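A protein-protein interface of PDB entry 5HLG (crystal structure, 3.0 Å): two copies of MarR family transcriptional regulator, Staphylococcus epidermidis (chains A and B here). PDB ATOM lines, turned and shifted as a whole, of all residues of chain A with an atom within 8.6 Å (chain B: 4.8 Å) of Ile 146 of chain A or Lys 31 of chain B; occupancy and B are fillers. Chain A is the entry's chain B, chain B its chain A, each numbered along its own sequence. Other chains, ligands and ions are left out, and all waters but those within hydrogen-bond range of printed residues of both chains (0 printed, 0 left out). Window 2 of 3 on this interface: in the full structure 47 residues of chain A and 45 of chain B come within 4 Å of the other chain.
NZ of Lys 31 of chain B is in hydrogen-bond range of O of Ile 146 of chain A.
Glu 139 of chain A touches Leu 24 of chain B (O to CD1, 3.6 Å).
Leu 142 of chain A touches Leu 24 of chain B.
CD1 of Leu 24 of chain B touches CG of Lys 143 of chain A (3.7 Å).
Ile 146 of chain A touches Leu 24 of chain B (CD1 to CD2, 3.4 Å).
Gln 27 of chain B touches Ile 146 of chain A.
Of chain B, only Leu 24, Gln 27 and Lys 31 come within 4 Å of Ile 146 of chain A.
Of the printed residues of chain B, Leu 142 of chain A touches Leu 24.
Of the printed residues of chain B, Lys 143 of chain A touches Leu 24 (3.7 Å).
Printed residues of chain B within 4 Å of Glu 139 of chain A: Leu 24 (3.6 Å).
Thr 141 of chain A touches none of the printed residues of chain B.
His 144 of chain A touches none of the printed residues of chain B.
The nearest residue of chain B that does not touch Ile 146 of chain A is Phe 28 of chain B (4.3 Å).
The nearest residue of chain A that does not touch Lys 31 of chain B is Glu 147 of chain A (5.2 Å).
The nearest printed residue of chain B that does not touch Glu 139 of chain A is Gln 27 of chain B (9.2 Å).
Of the 9 printed residues of chain B, 3 touch a printed residue of chain A.
Among the printed residues, no Asp or Glu carboxylate lies within 4 Å of a Lys or Arg side-chain nitrogen of the other chain.
No position is printed for both chains.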
ATOM      1  N   ASP A  65      11.688  16.011   9.722  1.00  0.00           N
ATOM      2  CA  ASP A  65      13.056  15.670  10.133  1.00  0.00           C
ATOM      3  C   ASP A  65      13.412  14.302   9.566  1.00  0.00           C
ATOM      4  O   ASP A  65      13.720  13.380  10.330  1.00  0.00           O
ATOM      5  CB  ASP A  65      13.266  15.683  11.666  1.00  0.00           C
ATOM      6  CG  ASP A  65      13.344  17.098  12.271  1.00  0.00           C
ATOM      7  OD1 ASP A  65      12.376  17.885  12.151  1.00  0.00           O
ATOM      8  OD2 ASP A  65      14.375  17.407  12.917  1.00  0.00           O
ATOM      9  N   GLU A 139      10.447  17.724  23.184  1.00  0.00           N
ATOM     10  CA  GLU A 139      10.894  17.669  21.793  1.00  0.00           C
ATOM     11  C   GLU A 139      11.983  18.711  21.556  1.00  0.00           C
ATOM     12  O   GLU A 139      13.051  18.393  21.050  1.00  0.00           O
ATOM     13  CB  GLU A 139       9.703  17.911  20.858  1.00  0.00           C
ATOM     14  CG  GLU A 139       9.930  17.538  19.402  1.00  0.00           C
ATOM     15  CD  GLU A 139       8.685  17.730  18.536  1.00  0.00           C
ATOM     16  OE1 GLU A 139       7.559  17.338  18.955  1.00  0.00           O
ATOM     17  OE2 GLU A 139       8.850  18.282  17.421  1.00  0.00           O
ATOM     18  N   GLN A 140      11.708  19.953  21.952  1.00  0.00           N
ATOM     19  CA  GLN A 140      12.682  21.039  21.855  1.00  0.00           C
ATOM     20  C   GLN A 140      13.883  20.870  22.762  1.00  0.00           C
ATOM     21  O   GLN A 140      14.988  21.239  22.390  1.00  0.00           O
ATOM     22  CB  GLN A 140      12.022  22.359  22.231  1.00  0.00           C
ATOM     23  CG  GLN A 140      11.138  22.987  21.120  1.00  0.00           C
ATOM     24  CD  GLN A 140      11.973  23.587  19.994  1.00  0.00           C
ATOM     25  OE1 GLN A 140      13.204  23.551  20.028  1.00  0.00           O
ATOM     26  NE2 GLN A 140      11.305  24.138  18.986  1.00  0.00           N
ATOM     27  N   THR A 141      13.664  20.359  23.967  1.00  0.00           N
ATOM     28  CA  THR A 141      14.765  20.096  24.890  1.00  0.00           C
ATOM     29  C   THR A 141      15.758  19.133  24.265  1.00  0.00           C
ATOM     30  O   THR A 141      16.968  19.395  24.245  1.00  0.00           O
ATOM     31  CB  THR A 141      14.258  19.480  26.208  1.00  0.00           C
ATOM     32  OG1 THR A 141      13.413  20.422  26.883  1.00  0.00           O
ATOM     33  CG2 THR A 141      15.418  19.107  27.125  1.00  0.00           C
ATOM     34  N   LEU A 142      15.231  18.023  23.748  1.00  0.00           N
ATOM     35  CA  LEU A 142      16.057  16.987  23.139  1.00  0.00           C
ATOM     36  C   LEU A 142      16.795  17.493  21.897  1.00  0.00           C
ATOM     37  O   LEU A 142      17.980  17.201  21.721  1.00  0.00           O
ATOM     38  CB  LEU A 142      15.208  15.759  22.803  1.00  0.00           C
ATOM     39  CG  LEU A 142      14.722  14.926  23.994  1.00  0.00           C
ATOM     40  CD1 LEU A 142      13.648  13.948  23.546  1.00  0.00           C
ATOM     41  CD2 LEU A 142      15.872  14.173  24.642  1.00  0.00           C
ATOM     42  N   LYS A 143      16.108  18.253  21.047  1.00  0.00           N
ATOM     43  CA  LYS A 143      16.744  18.841  19.846  1.00  0.00           C
ATOM     44  C   LYS A 143      17.991  19.669  20.124  1.00  0.00           C
ATOM     45  O   LYS A 143      18.907  19.705  19.310  1.00  0.00           O
ATOM     46  CB  LYS A 143      15.791  19.748  19.057  1.00  0.00           C
ATOM     47  CG  LYS A 143      14.741  19.000  18.259  1.00  0.00           C
ATOM     48  CD  LYS A 143      14.431  19.564  16.879  1.00  0.00           C
ATOM     49  CE  LYS A 143      13.012  20.060  16.791  1.00  0.00           C
ATOM     50  NZ  LYS A 143      12.667  20.360  15.381  1.00  0.00           N
ATOM     51  N   HIS A 144      17.990  20.388  21.237  1.00  0.00           N
ATOM     52  CA  HIS A 144      19.166  21.163  21.670  1.00  0.00           C
ATOM     53  C   HIS A 144      20.270  20.270  22.239  1.00  0.00           C
ATOM     54  O   HIS A 144      21.458  20.486  22.012  1.00  0.00           O
ATOM     55  CB  HIS A 144      18.742  22.222  22.692  1.00  0.00           C
ATOM     56  CG  HIS A 144      17.963  23.346  22.070  1.00  0.00           C
ATOM     57  ND1 HIS A 144      18.484  24.183  21.095  1.00  0.00           N
ATOM     58  CD2 HIS A 144      16.680  23.730  22.243  1.00  0.00           C
ATOM     59  CE1 HIS A 144      17.551  25.029  20.699  1.00  0.00           C
ATOM     60  NE2 HIS A 144      16.451  24.781  21.384  1.00  0.00           N
ATOM     61  N   LEU A 145      19.859  19.253  22.973  1.00  0.00           N
ATOM     62  CA  LEU A 145      20.776  18.265  23.531  1.00  0.00           C
ATOM     63  C   LEU A 145      21.602  17.531  22.469  1.00  0.00           C
ATOM     64  O   LEU A 145      22.681  17.042  22.778  1.00  0.00           O
ATOM     65  CB  LEU A 145      19.993  17.249  24.397  1.00  0.00           C
ATOM     66  CG  LEU A 145      19.837  17.345  25.915  1.00  0.00           C
ATOM     67  CD1 LEU A 145      19.486  15.982  26.493  1.00  0.00           C
ATOM     68  CD2 LEU A 145      21.090  17.878  26.562  1.00  0.00           C
ATOM     69  N   ILE A 146      21.103  17.449  21.233  1.00  0.00           N
ATOM     70  CA  ILE A 146      21.791  16.744  20.158  1.00  0.00           C
ATOM     71  C   ILE A 146      22.836  17.645  19.502  1.00  0.00           C
ATOM     72  O   ILE A 146      23.749  17.137  18.855  1.00  0.00           O
ATOM     73  CB  ILE A 146      20.782  16.192  19.117  1.00  0.00           C
ATOM     74  CG1 ILE A 146      19.778  15.280  19.827  1.00  0.00           C
ATOM     75  CG2 ILE A 146      21.491  15.436  17.995  1.00  0.00           C
ATOM     76  CD1 ILE A 146      18.877  14.473  18.917  1.00  0.00           C
ATOM     77  N   GLU A 147      22.718  18.965  19.678  1.00  0.00           N
ATOM     78  CA  GLU A 147      23.652  19.917  19.030  1.00  0.00           C
ATOM     79  C   GLU A 147      24.481  20.713  20.038  1.00  0.00           C
ATOM     80  O   GLU A 147      25.644  20.393  20.286  1.00  0.00           O
ATOM     81  CB  GLU A 147      22.919  20.854  18.057  1.00  0.00           C
ATOM     82  CG  GLU A 147      22.313  22.084  18.702  1.00  0.00           C
ATOM     83  CD  GLU A 147      21.138  22.646  17.926  1.00  0.00           C
ATOM     84  OE1 GLU A 147      20.919  22.215  16.771  1.00  0.00           O
ATOM     85  OE2 GLU A 147      20.427  23.516  18.480  1.00  0.00           O
ATOM     86  N   LEU B  24      14.427  11.306  18.569  1.00  0.00           N
ATOM     87  CA  LEU B  24      15.446  12.157  19.183  1.00  0.00           C
ATOM     88  C   LEU B  24      16.114  11.465  20.362  1.00  0.00           C
ATOM     89  O   LEU B  24      17.352  11.434  20.444  1.00  0.00           O
ATOM     90  CB  LEU B  24      14.850  13.498  19.609  1.00  0.00           C
ATOM     91  CG  LEU B  24      14.452  14.396  18.428  1.00  0.00           C
ATOM     92  CD1 LEU B  24      13.540  15.531  18.859  1.00  0.00           C
ATOM     93  CD2 LEU B  24      15.682  14.938  17.719  1.00  0.00           C
ATOM     94  N   GLN B  27      18.416   8.878  18.881  1.00  0.00           N
ATOM     95  CA  GLN B  27      19.576   9.575  18.329  1.00  0.00           C
ATOM     96  C   GLN B  27      20.584   9.959  19.399  1.00  0.00           C
ATOM     97  O   GLN B  27      21.768   9.698  19.259  1.00  0.00           O
ATOM     98  CB  GLN B  27      19.133  10.853  17.622  1.00  0.00           C
ATOM     99  CG  GLN B  27      19.226  10.819  16.114  1.00  0.00           C
ATOM    100  CD  GLN B  27      18.415  11.909  15.492  1.00  0.00           C
ATOM    101  OE1 GLN B  27      17.249  12.095  15.816  1.00  0.00           O
ATOM    102  NE2 GLN B  27      19.029  12.643  14.594  1.00  0.00           N
ATOM    103  N   PHE B  28      20.089  10.593  20.453  1.00  0.00           N
ATOM    104  CA  PHE B  28      20.901  11.019  21.567  1.00  0.00           C
ATOM    105  C   PHE B  28      21.614   9.822  22.198  1.00  0.00           C
ATOM    106  O   PHE B  28      22.851   9.766  22.192  1.00  0.00           O
ATOM    107  CB  PHE B  28      20.028  11.753  22.593  1.00  0.00           C
ATOM    108  CG  PHE B  28      20.739  12.075  23.868  1.00  0.00           C
ATOM    109  CD1 PHE B  28      21.611  13.152  23.941  1.00  0.00           C
ATOM    110  CD2 PHE B  28      20.549  11.296  24.995  1.00  0.00           C
ATOM    111  CE1 PHE B  28      22.278  13.449  25.118  1.00  0.00           C
ATOM    112  CE2 PHE B  28      21.210  11.586  26.174  1.00  0.00           C
ATOM    113  CZ  PHE B  28      22.073  12.662  26.237  1.00  0.00           C
ATOM    114  N   TYR B  29      20.842   8.863  22.713  1.00  0.00           N
ATOM    115  CA  TYR B  29      21.435   7.703  23.348  1.00  0.00           C
ATOM    116  C   TYR B  29      22.461   7.037  22.422  1.00  0.00           C
ATOM    117  O   TYR B  29      23.559   6.719  22.875  1.00  0.00           O
ATOM    118  CB  TYR B  29      20.353   6.725  23.828  1.00  0.00           C
ATOM    119  CG  TYR B  29      19.771   7.063  25.193  1.00  0.00           C
ATOM    120  CD1 TYR B  29      18.962   8.175  25.374  1.00  0.00           C
ATOM    121  CD2 TYR B  29      20.016   6.256  26.298  1.00  0.00           C
ATOM    122  CE1 TYR B  29      18.421   8.485  26.607  1.00  0.00           C
ATOM    123  CE2 TYR B  29      19.473   6.560  27.538  1.00  0.00           C
ATOM    124  CZ  TYR B  29      18.670   7.681  27.677  1.00  0.00           C
ATOM    125  OH  TYR B  29      18.105   8.028  28.881  1.00  0.00           O
ATOM    126  N   GLU B  30      22.139   6.895  21.130  1.00  0.00           N
ATOM    127  CA  GLU B  30      23.016   6.178  20.185  1.00  0.00           C
ATOM    128  C   GLU B  30      24.363   6.857  20.029  1.00  0.00           C
ATOM    129  O   GLU B  30      25.390   6.189  19.855  1.00  0.00           O
ATOM    130  CB  GLU B  30      22.366   6.042  18.803  1.00  0.00           C
ATOM    131  CG  GLU B  30      21.278   4.978  18.750  1.00  0.00           C
ATOM    132  CD  GLU B  30      21.522   3.907  17.703  1.00  0.00           C
ATOM    133  OE1 GLU B  30      22.009   4.245  16.600  1.00  0.00           O
ATOM    134  OE2 GLU B  30      21.194   2.733  17.983  1.00  0.00           O
ATOM    135  N   LYS B  31      24.340   8.185  20.072  1.00  0.00           N
ATOM    136  CA  LYS B  31      25.560   8.986  20.030  1.00  0.00           C
ATOM    137  C   LYS B  31      26.475   8.646  21.207  1.00  0.00           C
ATOM    138  O   LYS B  31      27.652   8.326  21.016  1.00  0.00           O
ATOM    139  CB  LYS B  31      25.215  10.480  20.057  1.00  0.00           C
ATOM    140  CG  LYS B  31      26.100  11.339  19.173  1.00  0.00           C
ATOM    141  CD  LYS B  31      25.670  12.797  19.279  1.00  0.00           C
ATOM    142  CE  LYS B  31      26.564  13.720  18.468  1.00  0.00           C
ATOM    143  NZ  LYS B  31      25.905  15.041  18.288  1.00  0.00           N
ATOM    144  N   LYS B  32      25.922   8.710  22.417  1.00  0.00           N
ATOM    145  CA  LYS B  32      26.687   8.431  23.627  1.00  0.00           C
ATOM    146  C   LYS B  32      27.126   6.972  23.685  1.00  0.00           C
ATOM    147  O   LYS B  32      28.242   6.682  24.106  1.00  0.00           O
ATOM    148  CB  LYS B  32      25.887   8.820  24.881  1.00  0.00           C
ATOM    149  CG  LYS B  32      25.342  10.246  24.881  1.00  0.00           C
ATOM    150  CD  LYS B  32      26.414  11.295  24.600  1.00  0.00           C
ATOM    151  CE  LYS B  32      25.800  12.640  24.229  1.00  0.00           C
ATOM    152  NZ  LYS B  32      26.807  13.559  23.624  1.00  0.00           N
ATOM    153  N   LEU B  33      26.280   6.066  23.200  1.00  0.00           N
ATOM    154  CA  LEU B  33      26.539   4.628  23.305  1.00  0.00           C
ATOM    155  C   LEU B  33      27.442   4.076  22.195  1.00  0.00           C
ATOM    156  O   LEU B  33      27.778   2.886  22.195  1.00  0.00           O
ATOM    157  CB  LEU B  33      25.220   3.855  23.295  1.00  0.00           C
ATOM    158  CG  LEU B  33      24.319   4.047  24.514  1.00  0.00           C
ATOM    159  CD1 LEU B  33      22.916   3.556  24.201  1.00  0.00           C
ATOM    160  CD2 LEU B  33      24.878   3.325  25.725  1.00  0.00           C
ATOM    161  N   LYS B  34      27.837   4.923  21.251  1.00  0.00           N
ATOM    162  CA  LYS B  34      28.622   4.446  20.118  1.00  0.00           C
ATOM    163  C   LYS B  34      29.971   3.877  20.575  1.00  0.00           C
ATOM    164  O   LYS B  34      30.428   2.863  20.037  1.00  0.00           O
ATOM    165  CB  LYS B  34      28.798   5.532  19.051  1.00  0.00           C
ATOM    166  CG  LYS B  34      28.713   4.978  17.641  1.00  0.00           C
ATOM    167  CD  LYS B  34      29.115   5.960  16.550  1.00  0.00           C
ATOM    168  CE  LYS B  34      29.050   5.290  15.184  1.00  0.00           C
ATOM    169  NZ  LYS B  34      29.425   6.217  14.082  1.00  0.00           N
